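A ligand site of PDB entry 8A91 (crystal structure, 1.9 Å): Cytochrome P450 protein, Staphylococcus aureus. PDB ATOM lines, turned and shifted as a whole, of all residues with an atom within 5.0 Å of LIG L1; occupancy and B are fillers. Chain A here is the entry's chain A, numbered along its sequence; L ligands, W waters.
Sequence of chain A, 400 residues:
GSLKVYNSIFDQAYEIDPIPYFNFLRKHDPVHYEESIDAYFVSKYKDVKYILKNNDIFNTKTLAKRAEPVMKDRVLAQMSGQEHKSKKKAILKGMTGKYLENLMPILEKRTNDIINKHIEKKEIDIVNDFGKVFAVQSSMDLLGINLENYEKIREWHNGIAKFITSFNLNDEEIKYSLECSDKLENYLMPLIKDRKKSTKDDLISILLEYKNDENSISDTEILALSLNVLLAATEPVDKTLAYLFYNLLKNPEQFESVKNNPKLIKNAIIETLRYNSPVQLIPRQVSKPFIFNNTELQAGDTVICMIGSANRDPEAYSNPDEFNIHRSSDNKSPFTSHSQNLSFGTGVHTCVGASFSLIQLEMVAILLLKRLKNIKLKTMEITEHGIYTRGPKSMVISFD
The backbone carbonyl oxygen (O) of Phe 344 is in hydrogen-bond range of the backbone NH (N) of Cys 351 (2.9 Å). A ring nitrogen (ND1) of His 349 sits at hydrogen-bond distance from a ring nitrogen (NE2) of His 84 (3.5 Å). The side-chain sulfur of Cys 351 sits close to the backbone NH of Gly 353 (3.3 Å). The side-chain hydroxyl (OG1) of Thr 350 lies within hydrogen-bond range of the backbone carbonyl oxygen (O) of Phe 344, at 2.9 Å. The backbone carbonyl oxygen (O) of Thr 350 is in hydrogen-bond range of the side-chain amino group (NZ) of Lys 88, at 2.8 Å. The side-chain hydroxyl of Ser 357 is in hydrogen-bond range of the backbone carbonyl oxygen of Gly 353, 2.5 Å away. O of Val 348 is in hydrogen-bond range of NZ of Lys 88, at 2.9 Å. The backbone NH (N) of Leu 76 lies close to the side-chain amide nitrogen (ND2) of Asn 228.
N1 of LG2 L2 is bound to FE1 of LIG L1.
The side-chain sulfur of Cys 351 binds an iron atom (FE1) of LIG L1 (2.2 Å). The backbone carbonyl oxygen of Ala 232 sits close to a nitrogen (N1) of LG2 L2 (3.4 Å). An oxygen (O2) of LIG L1 lies within salt-bridge range of the guanidinium group (NH2) of Arg 284, at 2.9 Å. A ring nitrogen (ND1) of His 349 sits at hydrogen-bond distance from an oxygen (O3) of LIG L1 (2.9 Å). The side-chain amino group of Lys 88 lies within salt-bridge range of an oxygen (O4) of LIG L1. A ring nitrogen (NE2) of His 84 sits at hydrogen-bond distance from an oxygen (O4) of LIG L1.
Residues that only touch LIG L1: Leu 63 (3.9 Å), Leu 76 (3.6 Å), Ala 77 (3.8 Å), Met 95 (3.2 Å), Val 229 (3.7 Å), Ala 232 (3.2 Å), Ala 233 (3.5 Å), Pro 236 (3.5 Å), Thr 240 (3.8 Å), Leu 273 (3.8 Å), Val 279 (3.9 Å), Ile 282 (3.5 Å), Ser 343 (3.2 Å), Phe 344 (3.5 Å), Gly 345 (3.4 Å), Val 348 (3.8 Å), Thr 350 (3.8 Å), Val 352 (3.5 Å), Gly 353 (3.8 Å), Phe 356 (3.95 Å) and Ser 357 (3.1 Å). Hydrophobic or aromatic side chains within 4 Å of LIG L1: Leu 63, Leu 76, His 84, Met 95, Val 229, Ala 232, Ala 233, Pro 236, Leu 273, Val 279, Ile 282, Phe 344, His 349, Val 352 and Phe 356. Within 4 Å of LIG L1: Leu 63, Leu 76, Ala 77, His 84, Lys 88, Met 95, Val 229, Ala 232, Ala 233, Pro 236, Thr 240, Leu 273, Val 279, Ile 282, Arg 284, Ser 343, Phe 344, Gly 345, Val 348, His 349, Thr 350, Cys 351, Val 352, Gly 353, Phe 356 and Ser 357. The nearest printed residue that does not touch LIG L1 is Pro 278 (4.3 Å).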
ATOM      1  N   LEU A  52      17.449   9.373  23.293  1.00  0.00           N
ATOM      2  CA  LEU A  52      16.710   9.425  22.035  1.00  0.00           C
ATOM      3  C   LEU A  52      16.450   8.037  21.456  1.00  0.00           C
ATOM      4  O   LEU A  52      15.475   7.859  20.714  1.00  0.00           O
ATOM      5  CB  LEU A  52      17.464  10.294  21.028  1.00  0.00           C
ATOM      6  CG  LEU A  52      17.616  11.767  21.397  1.00  0.00           C
ATOM      7  CD1 LEU A  52      18.498  12.507  20.394  1.00  0.00           C
ATOM      8  CD2 LEU A  52      16.250  12.442  21.512  1.00  0.00           C
ATOM      9  N   LEU A  63       6.304  17.453  24.451  1.00  0.00           N
ATOM     10  CA  LEU A  63       6.081  18.297  23.274  1.00  0.00           C
ATOM     11  C   LEU A  63       4.594  18.521  23.027  1.00  0.00           C
ATOM     12  O   LEU A  63       4.167  19.638  22.701  1.00  0.00           O
ATOM     13  CB  LEU A  63       6.739  17.654  22.060  1.00  0.00           C
ATOM     14  CG  LEU A  63       8.263  17.511  22.113  1.00  0.00           C
ATOM     15  CD1 LEU A  63       8.729  16.343  21.255  1.00  0.00           C
ATOM     16  CD2 LEU A  63       8.926  18.809  21.667  1.00  0.00           C
ATOM     17  N   LEU A  76       3.104  14.949  14.690  1.00  0.00           N
ATOM     18  CA  LEU A  76       3.800  13.681  14.518  1.00  0.00           C
ATOM     19  C   LEU A  76       4.452  13.222  15.815  1.00  0.00           C
ATOM     20  O   LEU A  76       4.433  12.026  16.138  1.00  0.00           O
ATOM     21  CB  LEU A  76       4.844  13.804  13.409  1.00  0.00           C
ATOM     22  CG  LEU A  76       5.320  12.500  12.776  1.00  0.00           C
ATOM     23  CD1 LEU A  76       4.153  11.723  12.181  1.00  0.00           C
ATOM     24  CD2 LEU A  76       6.402  12.756  11.730  1.00  0.00           C
ATOM     25  N   ALA A  77       5.046  14.146  16.564  1.00  0.00           N
ATOM     26  CA  ALA A  77       5.776  13.771  17.771  1.00  0.00           C
ATOM     27  C   ALA A  77       4.881  13.058  18.775  1.00  0.00           C
ATOM     28  O   ALA A  77       5.348  12.183  19.521  1.00  0.00           O
ATOM     29  CB  ALA A  77       6.414  15.002  18.409  1.00  0.00           C
ATOM     30  N   HIS A  84       2.285   6.445  13.818  1.00  0.00           N
ATOM     31  CA  HIS A  84       3.430   7.326  13.625  1.00  0.00           C
ATOM     32  C   HIS A  84       4.239   6.921  12.400  1.00  0.00           C
ATOM     33  O   HIS A  84       4.645   7.767  11.598  1.00  0.00           O
ATOM     34  CB  HIS A  84       4.313   7.325  14.875  1.00  0.00           C
ATOM     35  CG  HIS A  84       5.651   7.976  14.670  1.00  0.00           C
ATOM     36  ND1 HIS A  84       6.766   7.273  14.264  1.00  0.00           N
ATOM     37  CD2 HIS A  84       6.048   9.263  14.808  1.00  0.00           C
ATOM     38  CE1 HIS A  84       7.789   8.102  14.164  1.00  0.00           C
ATOM     39  NE2 HIS A  84       7.382   9.312  14.488  1.00  0.00           N
ATOM     40  N   LYS A  88       4.313   9.333   9.244  1.00  0.00           N
ATOM     41  CA  LYS A  88       5.670   9.810   8.945  1.00  0.00           C
ATOM     42  C   LYS A  88       6.066   9.434   7.519  1.00  0.00           C
ATOM     43  O   LYS A  88       6.749  10.212   6.837  1.00  0.00           O
ATOM     44  CB  LYS A  88       6.657   9.240   9.950  1.00  0.00           C
ATOM     45  CG  LYS A  88       8.091   9.740   9.771  1.00  0.00           C
ATOM     46  CD  LYS A  88       9.005   9.216  10.872  1.00  0.00           C
ATOM     47  CE  LYS A  88      10.270  10.046  10.979  1.00  0.00           C
ATOM     48  NZ  LYS A  88      11.032   9.759  12.228  1.00  0.00           N
ATOM     49  N   ILE A  91       4.412  11.936   5.077  1.00  0.00           N
ATOM     50  CA  ILE A  91       5.109  13.209   4.990  1.00  0.00           C
ATOM     51  C   ILE A  91       6.379  13.069   4.166  1.00  0.00           C
ATOM     52  O   ILE A  91       6.681  13.919   3.318  1.00  0.00           O
ATOM     53  CB  ILE A  91       5.402  13.768   6.394  1.00  0.00           C
ATOM     54  CG1 ILE A  91       4.113  14.246   7.062  1.00  0.00           C
ATOM     55  CG2 ILE A  91       6.424  14.892   6.315  1.00  0.00           C
ATOM     56  CD1 ILE A  91       4.255  14.552   8.533  1.00  0.00           C
ATOM     57  N   MET A  95       8.534  14.739  -0.044  1.00  0.00           N
ATOM     58  CA  MET A  95       9.880  15.233  -0.311  1.00  0.00           C
ATOM     59  C   MET A  95      10.747  14.151  -0.952  1.00  0.00           C
ATOM     60  O   MET A  95      11.984  14.247  -0.906  1.00  0.00           O
ATOM     61  CB  MET A  95      10.537  15.740   0.972  1.00  0.00           C
ATOM     62  CG  MET A  95      10.156  14.955   2.206  1.00  0.00           C
ATOM     63  SD  MET A  95      10.724  15.739   3.722  1.00  0.00           S
ATOM     64  CE  MET A  95       9.153  16.245   4.416  1.00  0.00           C
ATOM     65  N   LEU A 142       6.794  23.074  -0.725  1.00  0.00           N
ATOM     66  CA  LEU A 142       6.627  21.680  -0.291  1.00  0.00           C
ATOM     67  C   LEU A 142       5.171  21.381   0.032  1.00  0.00           C
ATOM     68  O   LEU A 142       4.615  20.369  -0.412  1.00  0.00           O
ATOM     69  CB  LEU A 142       7.521  21.410   0.914  1.00  0.00           C
ATOM     70  CG  LEU A 142       7.317  20.067   1.622  1.00  0.00           C
ATOM     71  CD1 LEU A 142       7.822  18.932   0.760  1.00  0.00           C
ATOM     72  CD2 LEU A 142       8.003  20.070   2.976  1.00  0.00           C
ATOM     73  N   ASN A 228       2.832  21.617  11.493  1.00  0.00           N
ATOM     74  CA  ASN A 228       4.006  20.895  11.955  1.00  0.00           C
ATOM     75  C   ASN A 228       5.139  20.966  10.928  1.00  0.00           C
ATOM     76  O   ASN A 228       6.285  21.266  11.272  1.00  0.00           O
ATOM     77  CB  ASN A 228       3.647  19.434  12.244  1.00  0.00           C
ATOM     78  CG  ASN A 228       4.763  18.666  12.910  1.00  0.00           C
ATOM     79  OD1 ASN A 228       5.809  19.225  13.236  1.00  0.00           O
ATOM     80  ND2 ASN A 228       4.547  17.377  13.125  1.00  0.00           N
ATOM     81  N   VAL A 229       4.814  20.705   9.656  1.00  0.00           N
ATOM     82  CA  VAL A 229       5.825  20.739   8.611  1.00  0.00           C
ATOM     83  C   VAL A 229       6.316  22.157   8.379  1.00  0.00           C
ATOM     84  O   VAL A 229       7.519  22.390   8.224  1.00  0.00           O
ATOM     85  CB  VAL A 229       5.272  20.099   7.326  1.00  0.00           C
ATOM     86  CG1 VAL A 229       6.179  20.413   6.146  1.00  0.00           C
ATOM     87  CG2 VAL A 229       5.120  18.599   7.505  1.00  0.00           C
ATOM     88  N   ALA A 232       8.632  22.857  11.199  1.00  0.00           N
ATOM     89  CA  ALA A 232       9.805  21.990  11.218  1.00  0.00           C
ATOM     90  C   ALA A 232      10.795  22.351  10.121  1.00  0.00           C
ATOM     91  O   ALA A 232      12.010  22.351  10.343  1.00  0.00           O
ATOM     92  CB  ALA A 232       9.371  20.528  11.092  1.00  0.00           C
ATOM     93  N   ALA A 233      10.290  22.668   8.930  1.00  0.00           N
ATOM     94  CA  ALA A 233      11.160  22.872   7.774  1.00  0.00           C
ATOM     95  C   ALA A 233      11.713  24.285   7.672  1.00  0.00           C
ATOM     96  O   ALA A 233      12.822  24.471   7.155  1.00  0.00           O
ATOM     97  CB  ALA A 233      10.403  22.539   6.485  1.00  0.00           C
ATOM     98  N   PRO A 236      15.047  25.785  10.819  1.00  0.00           N
ATOM     99  CA  PRO A 236      16.475  25.423  10.805  1.00  0.00           C
ATOM    100  C   PRO A 236      17.210  25.827   9.530  1.00  0.00           C
ATOM    101  O   PRO A 236      18.450  25.877   9.551  1.00  0.00           O
ATOM    102  CB  PRO A 236      16.450  23.896  10.948  1.00  0.00           C
ATOM    103  CG  PRO A 236      15.030  23.554  11.356  1.00  0.00           C
ATOM    104  CD  PRO A 236      14.187  24.601  10.724  1.00  0.00           C
ATOM    105  N   VAL A 237      16.508  26.126   8.439  1.00  0.00           N
ATOM    106  CA  VAL A 237      17.177  26.328   7.152  1.00  0.00           C
ATOM    107  C   VAL A 237      17.967  27.631   7.170  1.00  0.00           C
ATOM    108  O   VAL A 237      19.166  27.643   6.854  1.00  0.00           O
ATOM    109  CB  VAL A 237      16.153  26.311   6.005  1.00  0.00           C
ATOM    110  CG1 VAL A 237      16.696  27.037   4.788  1.00  0.00           C
ATOM    111  CG2 VAL A 237      15.785  24.874   5.666  1.00  0.00           C
ATOM    112  N   THR A 240      21.226  27.351   9.342  1.00  0.00           N
ATOM    113  CA  THR A 240      22.280  26.485   8.833  1.00  0.00           C
ATOM    114  C   THR A 240      22.985  27.117   7.631  1.00  0.00           C
ATOM    115  O   THR A 240      24.214  27.043   7.516  1.00  0.00           O
ATOM    116  CB  THR A 240      21.708  25.121   8.452  1.00  0.00           C
ATOM    117  OG1 THR A 240      21.136  24.514   9.615  1.00  0.00           O
ATOM    118  CG2 THR A 240      22.792  24.226   7.906  1.00  0.00           C
ATOM    119  N   LEU A 273      26.243  21.366  10.623  1.00  0.00           N
ATOM    120  CA  LEU A 273      25.161  20.954  11.503  1.00  0.00           C
ATOM    121  C   LEU A 273      25.698  20.406  12.819  1.00  0.00           C
ATOM    122  O   LEU A 273      25.062  20.588  13.870  1.00  0.00           O
ATOM    123  CB  LEU A 273      24.285  19.912  10.810  1.00  0.00           C
ATOM    124  CG  LEU A 273      23.470  20.467   9.636  1.00  0.00           C
ATOM    125  CD1 LEU A 273      22.854  19.333   8.822  1.00  0.00           C
ATOM    126  CD2 LEU A 273      22.388  21.415  10.142  1.00  0.00           C
ATOM    127  N   PRO A 278      21.626  23.908  14.704  1.00  0.00           N
ATOM    128  CA  PRO A 278      20.562  24.924  14.741  1.00  0.00           C
ATOM    129  C   PRO A 278      19.427  24.564  15.687  1.00  0.00           C
ATOM    130  O   PRO A 278      18.823  25.462  16.281  1.00  0.00           O
ATOM    131  CB  PRO A 278      20.087  24.990  13.281  1.00  0.00           C
ATOM    132  CG  PRO A 278      20.938  23.997  12.503  1.00  0.00           C
ATOM    133  CD  PRO A 278      21.578  23.085  13.495  1.00  0.00           C
ATOM    134  N   VAL A 279      19.120  23.278  15.835  1.00  0.00           N
ATOM    135  CA  VAL A 279      18.176  22.811  16.840  1.00  0.00           C
ATOM    136  C   VAL A 279      18.995  22.359  18.042  1.00  0.00           C
ATOM    137  O   VAL A 279      19.672  21.328  18.000  1.00  0.00           O
ATOM    138  CB  VAL A 279      17.285  21.679  16.313  1.00  0.00           C
ATOM    139  CG1 VAL A 279      16.318  21.211  17.396  1.00  0.00           C
ATOM    140  CG2 VAL A 279      16.524  22.146  15.072  1.00  0.00           C
ATOM    141  N   ILE A 282      16.252  19.056  22.640  1.00  0.00           N
ATOM    142  CA  ILE A 282      15.175  18.093  22.384  1.00  0.00           C
ATOM    143  C   ILE A 282      14.618  17.623  23.718  1.00  0.00           C
ATOM    144  O   ILE A 282      15.313  16.918  24.472  1.00  0.00           O
ATOM    145  CB  ILE A 282      15.664  16.903  21.552  1.00  0.00           C
ATOM    146  CG1 ILE A 282      16.104  17.339  20.161  1.00  0.00           C
ATOM    147  CG2 ILE A 282      14.572  15.855  21.438  1.00  0.00           C
ATOM    148  CD1 ILE A 282      16.743  16.231  19.343  1.00  0.00           C
ATOM    149  N   ARG A 284      12.234  15.449  26.392  1.00  0.00           N
ATOM    150  CA  ARG A 284      11.574  14.163  26.574  1.00  0.00           C
ATOM    151  C   ARG A 284      11.034  14.100  27.996  1.00  0.00           C
ATOM    152  O   ARG A 284      11.493  14.825  28.890  1.00  0.00           O
ATOM    153  CB  ARG A 284      12.523  12.987  26.323  1.00  0.00           C
ATOM    154  CG  ARG A 284      12.952  12.784  24.872  1.00  0.00           C
ATOM    155  CD  ARG A 284      11.776  12.409  23.993  1.00  0.00           C
ATOM    156  NE  ARG A 284      12.201  11.997  22.661  1.00  0.00           N
ATOM    157  CZ  ARG A 284      12.204  12.772  21.586  1.00  0.00           C
ATOM    158  NH1 ARG A 284      11.811  14.040  21.651  1.00  0.00           N
ATOM    159  NH2 ARG A 284      12.602  12.284  20.422  1.00  0.00           N
ATOM    160  N   LEU A 342      24.158  14.272  16.038  1.00  0.00           N
ATOM    161  CA  LEU A 342      22.778  14.205  16.486  1.00  0.00           C
ATOM    162  C   LEU A 342      21.958  15.403  16.020  1.00  0.00           C
ATOM    163  O   LEU A 342      20.902  15.680  16.587  1.00  0.00           O
ATOM    164  CB  LEU A 342      22.745  14.097  18.014  1.00  0.00           C
ATOM    165  CG  LEU A 342      23.369  12.818  18.598  1.00  0.00           C
ATOM    166  CD1 LEU A 342      23.742  13.007  20.062  1.00  0.00           C
ATOM    167  CD2 LEU A 342      22.434  11.645  18.422  1.00  0.00           C
ATOM    168  N   SER A 343      22.432  16.114  14.984  1.00  0.00           N
ATOM    169  CA  SER A 343      21.762  17.334  14.550  1.00  0.00           C
ATOM    170  C   SER A 343      20.344  17.078  14.063  1.00  0.00           C
ATOM    171  O   SER A 343      19.483  17.955  14.185  1.00  0.00           O
ATOM    172  CB  SER A 343      22.577  18.011  13.444  1.00  0.00           C
ATOM    173  OG  SER A 343      23.908  18.242  13.868  1.00  0.00           O
ATOM    174  N   PHE A 344      20.091  15.894  13.510  1.00  0.00           N
ATOM    175  CA  PHE A 344      18.753  15.485  13.095  1.00  0.00           C
ATOM    176  C   PHE A 344      18.099  14.548  14.098  1.00  0.00           C
ATOM    177  O   PHE A 344      17.113  13.881  13.768  1.00  0.00           O
ATOM    178  CB  PHE A 344      18.804  14.818  11.724  1.00  0.00           C
ATOM    179  CG  PHE A 344      19.173  15.743  10.594  1.00  0.00           C
ATOM    180  CD1 PHE A 344      18.311  16.749  10.182  1.00  0.00           C
ATOM    181  CD2 PHE A 344      20.387  15.601   9.930  1.00  0.00           C
ATOM    182  CE1 PHE A 344      18.645  17.595   9.140  1.00  0.00           C
ATOM    183  CE2 PHE A 344      20.719  16.438   8.882  1.00  0.00           C
ATOM    184  CZ  PHE A 344      19.856  17.440   8.494  1.00  0.00           C
ATOM    185  N   GLY A 345      18.620  14.481  15.319  1.00  0.00           N
ATOM    186  CA  GLY A 345      18.122  13.529  16.280  1.00  0.00           C
ATOM    187  C   GLY A 345      18.499  12.107  15.895  1.00  0.00           C
ATOM    188  O   GLY A 345      19.343  11.856  15.036  1.00  0.00           O
ATOM    189  N   VAL A 348      13.277   6.822  16.949  1.00  0.00           N
ATOM    190  CA  VAL A 348      11.961   6.784  16.320  1.00  0.00           C
ATOM    191  C   VAL A 348      11.588   8.122  15.701  1.00  0.00           C
ATOM    192  O   VAL A 348      11.003   8.178  14.621  1.00  0.00           O
ATOM    193  CB  VAL A 348      10.909   6.321  17.350  1.00  0.00           C
ATOM    194  CG1 VAL A 348       9.508   6.686  16.879  1.00  0.00           C
ATOM    195  CG2 VAL A 348      11.017   4.822  17.591  1.00  0.00           C
ATOM    196  N   HIS A 349      11.909   9.223  16.388  1.00  0.00           N
ATOM    197  CA  HIS A 349      11.472  10.548  15.963  1.00  0.00           C
ATOM    198  C   HIS A 349      12.567  11.332  15.239  1.00  0.00           C
ATOM    199  O   HIS A 349      12.497  12.565  15.188  1.00  0.00           O
ATOM    200  CB  HIS A 349      10.961  11.343  17.165  1.00  0.00           C
ATOM    201  CG  HIS A 349       9.726  10.761  17.787  1.00  0.00           C
ATOM    202  ND1 HIS A 349       8.465  11.011  17.297  1.00  0.00           N
ATOM    203  CD2 HIS A 349       9.565   9.954  18.865  1.00  0.00           C
ATOM    204  CE1 HIS A 349       7.573  10.368  18.043  1.00  0.00           C
ATOM    205  NE2 HIS A 349       8.213   9.730  18.999  1.00  0.00           N
ATOM    206  N   THR A 350      13.556  10.654  14.678  1.00  0.00           N
ATOM    207  CA  THR A 350      14.594  11.356  13.928  1.00  0.00           C
ATOM    208  C   THR A 350      13.966  12.129  12.778  1.00  0.00           C
ATOM    209  O   THR A 350      12.945  11.737  12.210  1.00  0.00           O
ATOM    210  CB  THR A 350      15.642  10.382  13.415  1.00  0.00           C
ATOM    211  OG1 THR A 350      16.775  11.110  12.915  1.00  0.00           O
ATOM    212  CG2 THR A 350      15.071   9.531  12.293  1.00  0.00           C
ATOM    213  N   CYS A 351      14.602  13.255  12.424  1.00  0.00           N
ATOM    214  CA  CYS A 351      14.005  14.202  11.494  1.00  0.00           C
ATOM    215  C   CYS A 351      13.624  13.528  10.173  1.00  0.00           C
ATOM    216  O   CYS A 351      14.470  12.928   9.507  1.00  0.00           O
ATOM    217  CB  CYS A 351      14.966  15.355  11.235  1.00  0.00           C
ATOM    218  SG  CYS A 351      14.333  16.551  10.034  1.00  0.00           S
ATOM    219  N   VAL A 352      12.344  13.646   9.803  1.00  0.00           N
ATOM    220  CA  VAL A 352      11.884  13.078   8.548  1.00  0.00           C
ATOM    221  C   VAL A 352      12.497  13.815   7.348  1.00  0.00           C
ATOM    222  O   VAL A 352      12.656  13.239   6.273  1.00  0.00           O
ATOM    223  CB  VAL A 352      10.352  13.097   8.480  1.00  0.00           C
ATOM    224  CG1 VAL A 352       9.847  14.521   8.287  1.00  0.00           C
ATOM    225  CG2 VAL A 352       9.848  12.196   7.357  1.00  0.00           C
ATOM    226  N   GLY A 353      12.848  15.080   7.530  1.00  0.00           N
ATOM    227  CA  GLY A 353      13.357  15.889   6.435  1.00  0.00           C
ATOM    228  C   GLY A 353      14.868  15.958   6.351  1.00  0.00           C
ATOM    229  O   GLY A 353      15.405  16.891   5.737  1.00  0.00           O
ATOM    230  N   PHE A 356      16.119  15.420   2.641  1.00  0.00           N
ATOM    231  CA  PHE A 356      15.694  16.576   1.857  1.00  0.00           C
ATOM    232  C   PHE A 356      16.487  17.822   2.235  1.00  0.00           C
ATOM    233  O   PHE A 356      16.933  18.577   1.355  1.00  0.00           O
ATOM    234  CB  PHE A 356      14.198  16.817   2.061  1.00  0.00           C
ATOM    235  CG  PHE A 356      13.697  18.072   1.404  1.00  0.00           C
ATOM    236  CD1 PHE A 356      13.702  18.202   0.028  1.00  0.00           C
ATOM    237  CD2 PHE A 356      13.212  19.125   2.165  1.00  0.00           C
ATOM    238  CE1 PHE A 356      13.235  19.358  -0.587  1.00  0.00           C
ATOM    239  CE2 PHE A 356      12.750  20.284   1.563  1.00  0.00           C
ATOM    240  CZ  PHE A 356      12.757  20.400   0.189  1.00  0.00           C
ATOM    241  N   SER A 357      16.683  18.056   3.529  1.00  0.00           N
ATOM    242  CA  SER A 357      17.429  19.232   3.966  1.00  0.00           C
ATOM    243  C   SER A 357      18.835  19.243   3.381  1.00  0.00           C
ATOM    244  O   SER A 357      19.322  20.292   2.935  1.00  0.00           O
ATOM    245  CB  SER A 357      17.483  19.278   5.498  1.00  0.00           C
ATOM    246  OG  SER A 357      16.188  19.248   6.060  1.00  0.00           O
ATOM    247  N   LEU A 361      19.981  22.136   0.882  1.00  0.00           N
ATOM    248  CA  LEU A 361      21.053  23.036   1.279  1.00  0.00           C
ATOM    249  C   LEU A 361      22.228  22.960   0.305  1.00  0.00           C
ATOM    250  O   LEU A 361      22.865  23.988   0.021  1.00  0.00           O
ATOM    251  CB  LEU A 361      21.520  22.700   2.701  1.00  0.00           C
ATOM    252  CG  LEU A 361      20.559  23.139   3.818  1.00  0.00           C
ATOM    253  CD1 LEU A 361      20.930  22.478   5.131  1.00  0.00           C
ATOM    254  CD2 LEU A 361      20.551  24.652   3.950  1.00  0.00           C
HETATM  255  C1  LIG L   1      12.287  16.149  13.775  1.00  0.00           C
HETATM  256  C2  LIG L   1      16.306  18.783  13.040  1.00  0.00           C
HETATM  257  C3  LIG L   1      14.657  20.020   8.645  1.00  0.00           C
HETATM  258  C4  LIG L   1      10.434  17.873   9.631  1.00  0.00           C
HETATM  259  C5  LIG L   1      13.533  16.721  13.954  1.00  0.00           C
HETATM  260  C6  LIG L   1      14.432  16.512  15.071  1.00  0.00           C
HETATM  261  C7  LIG L   1      15.537  17.229  14.859  1.00  0.00           C
HETATM  262  C8  LIG L   1      15.379  17.928  13.604  1.00  0.00           C
HETATM  263  C9  LIG L   1      16.765  17.315  15.795  1.00  0.00           C
HETATM  264  C10 LIG L   1      14.161  15.602  16.291  1.00  0.00           C
HETATM  265  C11 LIG L   1      13.086  16.190  17.198  1.00  0.00           C
HETATM  266  C12 LIG L   1      12.777  15.227  18.311  1.00  0.00           C
HETATM  267  O1  LIG L   1      11.919  15.540  19.173  1.00  0.00           O
HETATM  268  O2  LIG L   1      13.402  14.127  18.346  1.00  0.00           O
HETATM  269  C13 LIG L   1      16.229  19.325  11.773  1.00  0.00           C
HETATM  270  C14 LIG L   1      17.243  20.115  11.117  1.00  0.00           C
HETATM  271  C15 LIG L   1      16.782  20.462   9.905  1.00  0.00           C
HETATM  272  C16 LIG L   1      15.460  19.900   9.753  1.00  0.00           C
HETATM  273  C17 LIG L   1      18.602  20.462  11.771  1.00  0.00           C
HETATM  274  C18 LIG L   1      17.492  21.294   8.806  1.00  0.00           C
HETATM  275  C19 LIG L   1      18.796  21.556   8.860  1.00  0.00           C
HETATM  276  C20 LIG L   1      13.387  19.529   8.501  1.00  0.00           C
HETATM  277  C21 LIG L   1      12.583  19.580   7.297  1.00  0.00           C
HETATM  278  C22 LIG L   1      11.410  18.997   7.552  1.00  0.00           C
HETATM  279  C23 LIG L   1      11.430  18.534   8.934  1.00  0.00           C
HETATM  280  C24 LIG L   1      13.021  20.216   5.959  1.00  0.00           C
HETATM  281  C25 LIG L   1      10.275  18.851   6.513  1.00  0.00           C
HETATM  282  C26 LIG L   1       9.108  18.278   6.840  1.00  0.00           C
HETATM  283  C27 LIG L   1      10.567  17.207  10.828  1.00  0.00           C
HETATM  284  C28 LIG L   1       9.551  16.387  11.474  1.00  0.00           C
HETATM  285  C29 LIG L   1      10.069  15.916  12.617  1.00  0.00           C
HETATM  286  C30 LIG L   1      11.417  16.407  12.740  1.00  0.00           C
HETATM  287  C31 LIG L   1       8.129  16.112  10.947  1.00  0.00           C
HETATM  288  C32 LIG L   1       9.339  14.993  13.622  1.00  0.00           C
HETATM  289  C33 LIG L   1       9.844  13.576  13.402  1.00  0.00           C
HETATM  290  C34 LIG L   1       9.048  12.570  14.195  1.00  0.00           C
HETATM  291  O3  LIG L   1       8.398  12.966  15.193  1.00  0.00           O
HETATM  292  O4  LIG L   1       9.079  11.375  13.819  1.00  0.00           O
HETATM  293  N1  LIG L   1      14.154  17.589  13.074  1.00  0.00           N
HETATM  294  N2  LIG L   1      15.151  19.215  10.913  1.00  0.00           N
HETATM  295  N3  LIG L   1      12.648  18.880   9.474  1.00  0.00           N
HETATM  296  N4  LIG L   1      11.688  17.195  11.638  1.00  0.00           N
HETATM  297 FE1  LIG L   1      13.399  18.172  11.231  1.00  0.00          FE
HETATM  298  C1  LG2 L   2      13.309  20.682  13.013  1.00  0.00           C
HETATM  299  C2  LG2 L   2      11.213  24.115  16.572  1.00  0.00           C
HETATM  300  C3  LG2 L   2      12.921  20.944  14.440  1.00  0.00           C
HETATM  301  C4  LG2 L   2      12.120  21.948  16.345  1.00  0.00           C
HETATM  302  C5  LG2 L   2      12.333  22.151  14.963  1.00  0.00           C
HETATM  303  C6  LG2 L   2      11.957  23.374  14.401  1.00  0.00           C
HETATM  304  C7  LG2 L   2      13.034  20.095  15.498  1.00  0.00           C
HETATM  305  C8  LG2 L   2      11.564  22.928  17.160  1.00  0.00           C
HETATM  306  C9  LG2 L   2      11.409  24.347  15.207  1.00  0.00           C
HETATM  307  N1  LG2 L   2      12.432  19.701  12.357  1.00  0.00           N
HETATM  308  N2  LG2 L   2      12.556  20.678  16.639  1.00  0.00           N
HETATM  309  O   HOH W   1      11.507  17.960  19.723  1.00  0.00           O
HETATM  310  O   HOH W   2      15.949  21.965   5.335  1.00  0.00           O
HETATM  311  O   HOH W   3      15.339  12.093  17.471  1.00  0.00           O
